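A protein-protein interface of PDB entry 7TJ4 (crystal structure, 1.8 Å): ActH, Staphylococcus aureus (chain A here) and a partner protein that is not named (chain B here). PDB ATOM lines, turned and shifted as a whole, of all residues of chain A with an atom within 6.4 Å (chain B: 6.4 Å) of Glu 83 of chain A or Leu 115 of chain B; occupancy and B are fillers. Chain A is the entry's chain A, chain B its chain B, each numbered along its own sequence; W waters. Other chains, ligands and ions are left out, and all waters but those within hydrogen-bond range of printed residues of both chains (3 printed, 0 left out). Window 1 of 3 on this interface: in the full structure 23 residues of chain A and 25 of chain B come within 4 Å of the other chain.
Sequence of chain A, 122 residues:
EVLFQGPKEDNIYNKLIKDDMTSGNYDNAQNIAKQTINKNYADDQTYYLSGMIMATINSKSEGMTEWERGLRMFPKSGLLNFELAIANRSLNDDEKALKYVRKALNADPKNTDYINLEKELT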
ATOM      1  N   TYR A  48     -26.723  12.434 -32.202  1.00  0.00           N
ATOM      2  CA  TYR A  48     -26.820  12.536 -30.747  1.00  0.00           C
ATOM      3  C   TYR A  48     -25.442  12.501 -30.091  1.00  0.00           C
ATOM      4  O   TYR A  48     -25.060  13.431 -29.354  1.00  0.00           O
ATOM      5  CB  TYR A  48     -27.708  11.415 -30.216  1.00  0.00           C
ATOM      6  CG  TYR A  48     -27.664  11.273 -28.712  1.00  0.00           C
ATOM      7  CD1 TYR A  48     -28.406  12.136 -27.883  1.00  0.00           C
ATOM      8  CD2 TYR A  48     -26.893  10.296 -28.110  1.00  0.00           C
ATOM      9  CE1 TYR A  48     -28.366  12.040 -26.475  1.00  0.00           C
ATOM     10  CE2 TYR A  48     -26.864  10.183 -26.655  1.00  0.00           C
ATOM     11  CZ  TYR A  48     -27.618  11.074 -25.873  1.00  0.00           C
ATOM     12  OH  TYR A  48     -27.597  11.007 -24.492  1.00  0.00           O
ATOM     13  N   MET A  52     -23.308  15.380 -28.091  1.00  0.00           N
ATOM     14  CA  MET A  52     -22.896  15.136 -26.691  1.00  0.00           C
ATOM     15  C   MET A  52     -21.411  15.394 -26.519  1.00  0.00           C
ATOM     16  O   MET A  52     -20.971  15.953 -25.515  1.00  0.00           O
ATOM     17  CB  MET A  52     -23.188  13.690 -26.256  1.00  0.00           C
ATOM     18  CG  MET A  52     -24.628  13.359 -26.086  1.00  0.00           C
ATOM     19  SD  MET A  52     -25.416  14.270 -24.674  1.00  0.00           S
ATOM     20  CE  MET A  52     -24.832  13.300 -23.300  1.00  0.00           C
ATOM     21  N   ALA A  55     -21.054  19.130 -26.481  1.00  0.00           N
ATOM     22  CA  ALA A  55     -21.385  19.637 -25.150  1.00  0.00           C
ATOM     23  C   ALA A  55     -20.268  19.370 -24.138  1.00  0.00           C
ATOM     24  O   ALA A  55     -20.059  20.172 -23.220  1.00  0.00           O
ATOM     25  CB  ALA A  55     -22.699  19.034 -24.671  1.00  0.00           C
ATOM     26  N   LYS A  60     -22.488  23.678 -24.828  1.00  0.00           N
ATOM     27  CA  LYS A  60     -23.856  23.194 -24.992  1.00  0.00           C
ATOM     28  C   LYS A  60     -24.473  23.737 -26.272  1.00  0.00           C
ATOM     29  O   LYS A  60     -25.180  23.012 -26.986  1.00  0.00           O
ATOM     30  CB  LYS A  60     -24.735  23.601 -23.813  1.00  0.00           C
ATOM     31  CG  LYS A  60     -26.130  23.016 -23.934  1.00  0.00           C
ATOM     32  CD  LYS A  60     -27.036  23.239 -22.678  1.00  0.00           C
ATOM     33  CE  LYS A  60     -26.546  24.318 -21.725  1.00  0.00           C
ATOM     34  NZ  LYS A  60     -27.569  24.438 -20.619  1.00  0.00           N
ATOM     35  N   MET A  64     -26.218  21.614 -29.266  1.00  0.00           N
ATOM     36  CA  MET A  64     -27.598  21.765 -29.695  1.00  0.00           C
ATOM     37  C   MET A  64     -27.668  21.989 -31.204  1.00  0.00           C
ATOM     38  O   MET A  64     -28.551  21.447 -31.873  1.00  0.00           O
ATOM     39  CB  MET A  64     -28.250  22.909 -28.915  1.00  0.00           C
ATOM     40  CG  MET A  64     -28.634  22.508 -27.513  1.00  0.00           C
ATOM     41  SD  MET A  64     -29.109  23.917 -26.533  1.00  0.00           S
ATOM     42  CE  MET A  64     -30.734  24.359 -27.131  1.00  0.00           C
ATOM     43  N   TRP A  67     -27.439  18.558 -32.712  1.00  0.00           N
ATOM     44  CA  TRP A  67     -28.667  17.785 -32.614  1.00  0.00           C
ATOM     45  C   TRP A  67     -29.725  18.297 -33.578  1.00  0.00           C
ATOM     46  O   TRP A  67     -30.494  17.495 -34.122  1.00  0.00           O
ATOM     47  CB  TRP A  67     -29.215  17.771 -31.189  1.00  0.00           C
ATOM     48  CG  TRP A  67     -28.279  17.114 -30.220  1.00  0.00           C
ATOM     49  CD1 TRP A  67     -27.470  16.019 -30.443  1.00  0.00           C
ATOM     50  CD2 TRP A  67     -28.014  17.534 -28.881  1.00  0.00           C
ATOM     51  NE1 TRP A  67     -26.737  15.738 -29.312  1.00  0.00           N
ATOM     52  CE2 TRP A  67     -27.067  16.646 -28.338  1.00  0.00           C
ATOM     53  CE3 TRP A  67     -28.496  18.582 -28.082  1.00  0.00           C
ATOM     54  CZ2 TRP A  67     -26.567  16.786 -27.022  1.00  0.00           C
ATOM     55  CZ3 TRP A  67     -27.999  18.711 -26.777  1.00  0.00           C
ATOM     56  CH2 TRP A  67     -27.054  17.816 -26.276  1.00  0.00           C
ATOM     57  N   GLY A  78     -36.864  10.190 -31.678  1.00  0.00           N
ATOM     58  CA  GLY A  78     -37.184  10.449 -30.284  1.00  0.00           C
ATOM     59  C   GLY A  78     -35.956  10.857 -29.483  1.00  0.00           C
ATOM     60  O   GLY A  78     -36.014  11.790 -28.679  1.00  0.00           O
ATOM     61  N   LEU A  79     -34.831  10.177 -29.716  1.00  0.00           N
ATOM     62  CA  LEU A  79     -33.546  10.504 -29.089  1.00  0.00           C
ATOM     63  C   LEU A  79     -33.194  11.976 -29.242  1.00  0.00           C
ATOM     64  O   LEU A  79     -32.908  12.669 -28.254  1.00  0.00           O
ATOM     65  CB  LEU A  79     -32.445   9.629 -29.695  1.00  0.00           C
ATOM     66  CG  LEU A  79     -31.027   9.653 -29.127  1.00  0.00           C
ATOM     67  CD1 LEU A  79     -31.047   9.241 -27.667  1.00  0.00           C
ATOM     68  CD2 LEU A  79     -30.177   8.676 -29.896  1.00  0.00           C
ATOM     69  N   LEU A  80     -33.193  12.475 -30.480  1.00  0.00           N
ATOM     70  CA  LEU A  80     -32.760  13.842 -30.703  1.00  0.00           C
ATOM     71  C   LEU A  80     -33.809  14.840 -30.230  1.00  0.00           C
ATOM     72  O   LEU A  80     -33.459  15.932 -29.767  1.00  0.00           O
ATOM     73  CB  LEU A  80     -32.440  14.079 -32.186  1.00  0.00           C
ATOM     74  CG  LEU A  80     -31.293  13.263 -32.768  1.00  0.00           C
ATOM     75  CD1 LEU A  80     -31.402  13.258 -34.331  1.00  0.00           C
ATOM     76  CD2 LEU A  80     -29.944  13.879 -32.306  1.00  0.00           C
ATOM     77  N   ASN A  81     -35.097  14.506 -30.388  1.00  0.00           N
ATOM     78  CA  ASN A  81     -36.134  15.417 -29.937  1.00  0.00           C
ATOM     79  C   ASN A  81     -36.149  15.486 -28.416  1.00  0.00           C
ATOM     80  O   ASN A  81     -36.302  16.569 -27.848  1.00  0.00           O
ATOM     81  CB  ASN A  81     -37.496  15.000 -30.475  1.00  0.00           C
ATOM     82  CG  ASN A  81     -37.715  15.476 -31.907  1.00  0.00           C
ATOM     83  OD1 ASN A  81     -37.731  16.690 -32.173  1.00  0.00           O
ATOM     84  ND2 ASN A  81     -37.910  14.537 -32.818  1.00  0.00           N
ATOM     85  N   PHE A  82     -35.986  14.350 -27.748  1.00  0.00           N
ATOM     86  CA  PHE A  82     -35.947  14.379 -26.293  1.00  0.00           C
ATOM     87  C   PHE A  82     -34.748  15.167 -25.819  1.00  0.00           C
ATOM     88  O   PHE A  82     -34.854  16.021 -24.918  1.00  0.00           O
ATOM     89  CB  PHE A  82     -35.914  12.965 -25.726  1.00  0.00           C
ATOM     90  CG  PHE A  82     -36.153  12.895 -24.223  1.00  0.00           C
ATOM     91  CD1 PHE A  82     -37.306  13.405 -23.674  1.00  0.00           C
ATOM     92  CD2 PHE A  82     -35.221  12.295 -23.378  1.00  0.00           C
ATOM     93  CE1 PHE A  82     -37.520  13.328 -22.264  1.00  0.00           C
ATOM     94  CE2 PHE A  82     -35.434  12.201 -21.987  1.00  0.00           C
ATOM     95  CZ  PHE A  82     -36.577  12.723 -21.426  1.00  0.00           C
ATOM     96  N   GLU A  83     -33.601  14.935 -26.446  1.00  0.00           N
ATOM     97  CA  GLU A  83     -32.399  15.609 -25.975  1.00  0.00           C
ATOM     98  C   GLU A  83     -32.521  17.110 -26.139  1.00  0.00           C
ATOM     99  O   GLU A  83     -32.060  17.881 -25.278  1.00  0.00           O
ATOM    100  CB  GLU A  83     -31.162  15.080 -26.706  1.00  0.00           C
ATOM    101  CG  GLU A  83     -29.853  15.541 -26.014  1.00  0.00           C
ATOM    102  CD  GLU A  83     -29.670  15.014 -24.541  1.00  0.00           C
ATOM    103  OE1 GLU A  83     -30.221  13.953 -24.170  1.00  0.00           O
ATOM    104  OE2 GLU A  83     -28.954  15.673 -23.755  1.00  0.00           O
ATOM    105  N   LEU A  84     -33.143  17.558 -27.240  1.00  0.00           N
ATOM    106  CA  LEU A  84     -33.327  18.990 -27.409  1.00  0.00           C
ATOM    107  C   LEU A  84     -34.413  19.532 -26.494  1.00  0.00           C
ATOM    108  O   LEU A  84     -34.397  20.711 -26.188  1.00  0.00           O
ATOM    109  CB  LEU A  84     -33.649  19.342 -28.868  1.00  0.00           C
ATOM    110  CG  LEU A  84     -32.401  19.524 -29.753  1.00  0.00           C
ATOM    111  CD1 LEU A  84     -32.718  19.382 -31.260  1.00  0.00           C
ATOM    112  CD2 LEU A  84     -31.819  20.876 -29.488  1.00  0.00           C
ATOM    113  N   ALA A  85     -35.398  18.723 -26.105  1.00  0.00           N
ATOM    114  CA  ALA A  85     -36.325  19.169 -25.068  1.00  0.00           C
ATOM    115  C   ALA A  85     -35.578  19.389 -23.758  1.00  0.00           C
ATOM    116  O   ALA A  85     -35.762  20.413 -23.097  1.00  0.00           O
ATOM    117  CB  ALA A  85     -37.465  18.170 -24.867  1.00  0.00           C
ATOM    118  N   ILE A  86     -34.726  18.442 -23.366  1.00  0.00           N
ATOM    119  CA  ILE A  86     -33.943  18.619 -22.138  1.00  0.00           C
ATOM    120  C   ILE A  86     -33.095  19.880 -22.224  1.00  0.00           C
ATOM    121  O   ILE A  86     -33.071  20.720 -21.307  1.00  0.00           O
ATOM    122  CB  ILE A  86     -33.052  17.395 -21.891  1.00  0.00           C
ATOM    123  CG1 ILE A  86     -33.898  16.165 -21.615  1.00  0.00           C
ATOM    124  CG2 ILE A  86     -32.093  17.693 -20.663  1.00  0.00           C
ATOM    125  CD1 ILE A  86     -33.066  14.896 -21.604  1.00  0.00           C
ATOM    126  N   ALA A  87     -32.366  20.020 -23.328  1.00  0.00           N
ATOM    127  CA  ALA A  87     -31.492  21.178 -23.495  1.00  0.00           C
ATOM    128  C   ALA A  87     -32.275  22.474 -23.414  1.00  0.00           C
ATOM    129  O   ALA A  87     -31.813  23.439 -22.805  1.00  0.00           O
ATOM    130  CB  ALA A  87     -30.752  21.081 -24.839  1.00  0.00           C
ATOM    131  N   ASN A  88     -33.457  22.540 -24.052  1.00  0.00           N
ATOM    132  CA  ASN A  88     -34.157  23.814 -24.023  1.00  0.00           C
ATOM    133  C   ASN A  88     -34.729  24.100 -22.638  1.00  0.00           C
ATOM    134  O   ASN A  88     -34.816  25.271 -22.227  1.00  0.00           O
ATOM    135  CB  ASN A  88     -35.232  23.870 -25.105  1.00  0.00           C
ATOM    136  CG  ASN A  88     -34.656  24.297 -26.441  1.00  0.00           C
ATOM    137  OD1 ASN A  88     -34.369  25.474 -26.644  1.00  0.00           O
ATOM    138  ND2 ASN A  88     -34.385  23.333 -27.303  1.00  0.00           N
ATOM    139  N   ARG A  89     -35.116  23.053 -21.908  1.00  0.00           N
ATOM    140  CA  ARG A  89     -35.469  23.244 -20.507  1.00  0.00           C
ATOM    141  C   ARG A  89     -34.298  23.840 -19.733  1.00  0.00           C
ATOM    142  O   ARG A  89     -34.495  24.737 -18.924  1.00  0.00           O
ATOM    143  CB  ARG A  89     -35.921  21.927 -19.879  1.00  0.00           C
ATOM    144  CG  ARG A  89     -36.293  22.025 -18.408  1.00  0.00           C
ATOM    145  CD  ARG A  89     -36.707  20.653 -17.890  1.00  0.00           C
ATOM    146  NE  ARG A  89     -35.562  19.802 -17.599  1.00  0.00           N
ATOM    147  CZ  ARG A  89     -35.487  18.961 -16.572  1.00  0.00           C
ATOM    148  NH1 ARG A  89     -36.500  18.814 -15.719  1.00  0.00           N
ATOM    149  NH2 ARG A  89     -34.364  18.262 -16.385  1.00  0.00           N
ATOM    150  N   SER A  90     -33.061  23.401 -20.018  1.00  0.00           N
ATOM    151  CA  SER A  90     -31.939  23.909 -19.243  1.00  0.00           C
ATOM    152  C   SER A  90     -31.658  25.364 -19.550  1.00  0.00           C
ATOM    153  O   SER A  90     -31.081  26.060 -18.703  1.00  0.00           O
ATOM    154  CB  SER A  90     -30.684  23.096 -19.461  1.00  0.00           C
ATOM    155  OG  SER A  90     -30.155  23.374 -20.754  1.00  0.00           O
ATOM    156  N   ILE B 110     -20.168  25.227 -15.341  1.00  0.00           N
ATOM    157  CA  ILE B 110     -21.111  24.133 -15.487  1.00  0.00           C
ATOM    158  C   ILE B 110     -22.288  24.577 -16.342  1.00  0.00           C
ATOM    159  O   ILE B 110     -22.820  23.810 -17.137  1.00  0.00           O
ATOM    160  CB  ILE B 110     -21.576  23.613 -14.126  1.00  0.00           C
ATOM    161  CG1 ILE B 110     -20.405  22.989 -13.342  1.00  0.00           C
ATOM    162  CG2 ILE B 110     -22.648  22.613 -14.382  1.00  0.00           C
ATOM    163  CD1 ILE B 110     -20.696  22.802 -11.796  1.00  0.00           C
ATOM    164  N   LYS B 113     -22.042  24.096 -20.233  1.00  0.00           N
ATOM    165  CA  LYS B 113     -21.939  22.788 -20.869  1.00  0.00           C
ATOM    166  C   LYS B 113     -23.009  21.831 -20.401  1.00  0.00           C
ATOM    167  O   LYS B 113     -23.518  21.056 -21.216  1.00  0.00           O
ATOM    168  CB  LYS B 113     -20.544  22.180 -20.613  1.00  0.00           C
ATOM    169  CG  LYS B 113     -19.414  22.784 -21.465  1.00  0.00           C
ATOM    170  CD  LYS B 113     -18.093  22.130 -21.097  1.00  0.00           C
ATOM    171  CE  LYS B 113     -16.981  22.597 -22.015  1.00  0.00           C
ATOM    172  NZ  LYS B 113     -15.737  21.823 -21.783  1.00  0.00           N
ATOM    173  N   GLY B 114     -23.366  21.871 -19.119  1.00  0.00           N
ATOM    174  CA  GLY B 114     -24.270  20.882 -18.580  1.00  0.00           C
ATOM    175  C   GLY B 114     -25.687  21.083 -19.077  1.00  0.00           C
ATOM    176  O   GLY B 114     -26.096  22.178 -19.418  1.00  0.00           O
ATOM    177  N   LEU B 115     -26.443  19.994 -19.106  1.00  0.00           N
ATOM    178  CA  LEU B 115     -27.826  20.009 -19.562  1.00  0.00           C
ATOM    179  C   LEU B 115     -28.805  20.189 -18.411  1.00  0.00           C
ATOM    180  O   LEU B 115     -30.007  19.961 -18.585  1.00  0.00           O
ATOM    181  CB  LEU B 115     -28.144  18.714 -20.320  1.00  0.00           C
ATOM    182  CG  LEU B 115     -27.774  18.575 -21.814  1.00  0.00           C
ATOM    183  CD1 LEU B 115     -28.382  19.628 -22.597  1.00  0.00           C
ATOM    184  CD2 LEU B 115     -26.343  18.705 -21.991  1.00  0.00           C
ATOM    185  N   LEU B 116     -28.313  20.591 -17.233  1.00  0.00           N
ATOM    186  CA  LEU B 116     -29.187  20.872 -16.092  1.00  0.00           C
ATOM    187  C   LEU B 116     -29.559  22.346 -16.097  1.00  0.00           C
ATOM    188  O   LEU B 116     -28.757  23.182 -16.486  1.00  0.00           O
ATOM    189  CB  LEU B 116     -28.482  20.512 -14.787  1.00  0.00           C
ATOM    190  CG  LEU B 116     -28.153  19.015 -14.724  1.00  0.00           C
ATOM    191  CD1 LEU B 116     -27.276  18.669 -13.498  1.00  0.00           C
ATOM    192  CD2 LEU B 116     -29.430  18.232 -14.664  1.00  0.00           C
ATOM    193  N   SER B 117     -30.781  22.658 -15.656  1.00  0.00           N
ATOM    194  CA  SER B 117     -31.157  24.029 -15.361  1.00  0.00           C
ATOM    195  C   SER B 117     -30.239  24.638 -14.280  1.00  0.00           C
ATOM    196  O   SER B 117     -29.888  23.983 -13.316  1.00  0.00           O
ATOM    197  CB  SER B 117     -32.606  24.071 -14.883  1.00  0.00           C
ATOM    198  OG  SER B 117     -33.472  23.571 -15.893  1.00  0.00           O
ATOM    199  N   ASP B 149     -34.221  14.958 -14.710  1.00  0.00           N
ATOM    200  CA  ASP B 149     -32.879  14.944 -14.117  1.00  0.00           C
ATOM    201  C   ASP B 149     -32.399  13.518 -13.873  1.00  0.00           C
ATOM    202  O   ASP B 149     -31.240  13.183 -14.133  1.00  0.00           O
ATOM    203  CB  ASP B 149     -32.859  15.701 -12.780  1.00  0.00           C
ATOM    204  CG  ASP B 149     -32.805  17.213 -12.934  1.00  0.00           C
ATOM    205  OD1 ASP B 149     -32.860  17.762 -14.066  1.00  0.00           O
ATOM    206  OD2 ASP B 149     -32.668  17.885 -11.885  1.00  0.00           O
ATOM    207  N   MET B 152     -30.811  11.865 -16.640  1.00  0.00           N
ATOM    208  CA  MET B 152     -29.416  12.260 -16.877  1.00  0.00           C
ATOM    209  C   MET B 152     -28.452  11.826 -15.779  1.00  0.00           C
ATOM    210  O   MET B 152     -27.302  11.475 -16.058  1.00  0.00           O
ATOM    211  CB  MET B 152     -29.311  13.761 -17.058  1.00  0.00           C
ATOM    212  CG  MET B 152     -30.087  14.283 -18.253  1.00  0.00           C
ATOM    213  SD  MET B 152     -29.872  16.051 -18.449  1.00  0.00           S
ATOM    214  CE  MET B 152     -31.199  16.761 -17.475  1.00  0.00           C
ATOM    215  N   HIS B 158     -24.122  11.899 -19.944  1.00  0.00           N
ATOM    216  CA  HIS B 158     -24.473  13.188 -19.338  1.00  0.00           C
ATOM    217  C   HIS B 158     -23.601  13.516 -18.137  1.00  0.00           C
ATOM    218  O   HIS B 158     -23.131  14.640 -18.026  1.00  0.00           O
ATOM    219  CB  HIS B 158     -25.936  13.224 -18.938  1.00  0.00           C
ATOM    220  CG  HIS B 158     -26.849  13.411 -20.094  1.00  0.00           C
ATOM    221  ND1 HIS B 158     -27.279  12.360 -20.883  1.00  0.00           N
ATOM    222  CD2 HIS B 158     -27.349  14.536 -20.652  1.00  0.00           C
ATOM    223  CE1 HIS B 158     -28.050  12.835 -21.850  1.00  0.00           C
ATOM    224  NE2 HIS B 158     -28.109  14.152 -21.730  1.00  0.00           N
ATOM    225  N   ILE B 161     -20.331  15.111 -19.108  1.00  0.00           N
ATOM    226  CA  ILE B 161     -20.381  16.517 -19.494  1.00  0.00           C
ATOM    227  C   ILE B 161     -20.205  17.385 -18.244  1.00  0.00           C
ATOM    228  O   ILE B 161     -19.450  18.357 -18.228  1.00  0.00           O
ATOM    229  CB  ILE B 161     -21.722  16.849 -20.169  1.00  0.00           C
ATOM    230  CG1 ILE B 161     -21.923  16.235 -21.569  1.00  0.00           C
ATOM    231  CG2 ILE B 161     -21.903  18.350 -20.259  1.00  0.00           C
ATOM    232  CD1 ILE B 161     -23.362  16.500 -22.010  1.00  0.00           C
ATOM    233  N   LEU B 162     -21.004  17.093 -17.232  1.00  0.00           N
ATOM    234  CA  LEU B 162     -20.877  17.729 -15.915  1.00  0.00           C
ATOM    235  C   LEU B 162     -19.472  17.601 -15.383  1.00  0.00           C
ATOM    236  O   LEU B 162     -18.892  18.573 -14.881  1.00  0.00           O
ATOM    237  CB  LEU B 162     -21.863  17.084 -14.953  1.00  0.00           C
ATOM    238  CG  LEU B 162     -23.327  17.311 -15.352  1.00  0.00           C
ATOM    239  CD1 LEU B 162     -24.309  16.823 -14.265  1.00  0.00           C
ATOM    240  CD2 LEU B 162     -23.576  18.765 -15.627  1.00  0.00           C
HETATM  241  O   HOH W   1     -32.430  20.276 -15.024  1.00  0.00           O
HETATM  242  O   HOH W   2     -34.354  26.712 -16.573  1.00  0.00           O
HETATM  243  O   HOH W   3     -32.668  20.156 -18.277  1.00  0.00           O
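Printed residues of chain B that touch a printed residue of chain A: Lys 113, Gly 114, Leu 115, Leu 116, Ser 117, Asp 149, Met 152, His 158 and Ile 161. Hydrophobic or aromatic side chains of chain B that line the printed part of chain A: Leu 115, Met 152, His 158 and Ile 161.
Among the printed residues, merely in contact across the chains: Tyr 48 of chain A with His 158 of chain B, Met 52 of chain A with His 158 of chain B, Met 52 of chain A with Ile 161 of chain B, Ala 55 of chain A with Lys 113 of chain B, Ala 55 of chain A with Ile 161 of chain B, Lys 60 of chain A with Lys 113 of chain B, Lys 60 of chain A with Leu 115 of chain B, Glu 83 of chain A with Leu 115 of chain B, Ile 86 of chain A with Leu 115 of chain B, Ile 86 of chain A with Met 152 of chain B, Ala 87 of chain A with Leu 115 of chain B, Arg 89 of chain A with Met 152 of chain B, Ser 90 of chain A with Leu 115 of chain B, Ser 90 of chain A with Leu 116 of chain B and Ser 90 of chain A with Ser 117 of chain B.
Glu 83 of chain A touches two residues of chain B. Of the printed residues of chain B, Arg 89 of chain A touches Ser 117 (3.4 Å), Asp 149 (2.8 Å) and Met 152 (3.7 Å). Of the printed residues of chain A, Gly 114 of chain B touches Lys 60. Of chain A, only Lys 60 (3.9 Å), Glu 83 (3.7 Å), Ile 86 (3.7 Å), Ala 87 (3.6 Å) and Ser 90 (3.3 Å) come within 4 Å of Leu 115 of chain B. The nearest residue of chain B that does not touch Glu 83 of chain A is Met 152 of chain B (5.4 Å). The nearest residue of chain A that does not touch Leu 115 of chain B is Trp 67 of chain A (4.3 Å).
NE1 of Trp 67 of chain A sits at hydrogen-bond distance from O of Tyr 48 of chain A, 2.9 Å away. The side-chain amino group of Lys 60 of chain A sits at hydrogen-bond distance from the side-chain hydroxyl of Ser 90 of chain A, 2.8 Å away. The backbone carbonyl oxygen (O) of Ala 87 of chain A is in hydrogen-bond range of the side-chain hydroxyl (OG) of Ser 90 of chain A, 2.6 Å away.
Water W3 lies within hydrogen-bond range of O of Leu 115 of chain B (2.7 Å), NE of Arg 89 of chain A (3.0 Å) and O of Ile 86 of chain A (3.1 Å). Water W1 lies within hydrogen-bond range of the side-chain carboxylate (OD1) of Asp 149 of chain B (2.7 Å), the backbone NH (N) of Ser 117 of chain B (3.0 Å) and the guanidinium group (NH2) of Arg 89 of chain A (3.1 Å). Water W2 bridges the backbone carbonyl oxygen of Arg 89 of chain A (3.1 Å) and the side-chain hydroxyl of Ser 117 of chain B (3.3 Å).
NZ of Lys 60 of chain A sits at hydrogen-bond distance from O of Gly 114 of chain B (3.0 Å). OE2 of Glu 83 of chain A is in hydrogen-bond range of NE2 of His 158 of chain B. The backbone carbonyl oxygen (O) of Arg 89 of chain A sits at hydrogen-bond distance from the side-chain hydroxyl (OG) of Ser 117 of chain B (3.4 Å). The side-chain carboxylate of Asp 149 of chain B lies within salt-bridge range of the guanidinium group of Arg 89 of chain A (2.8 Å).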
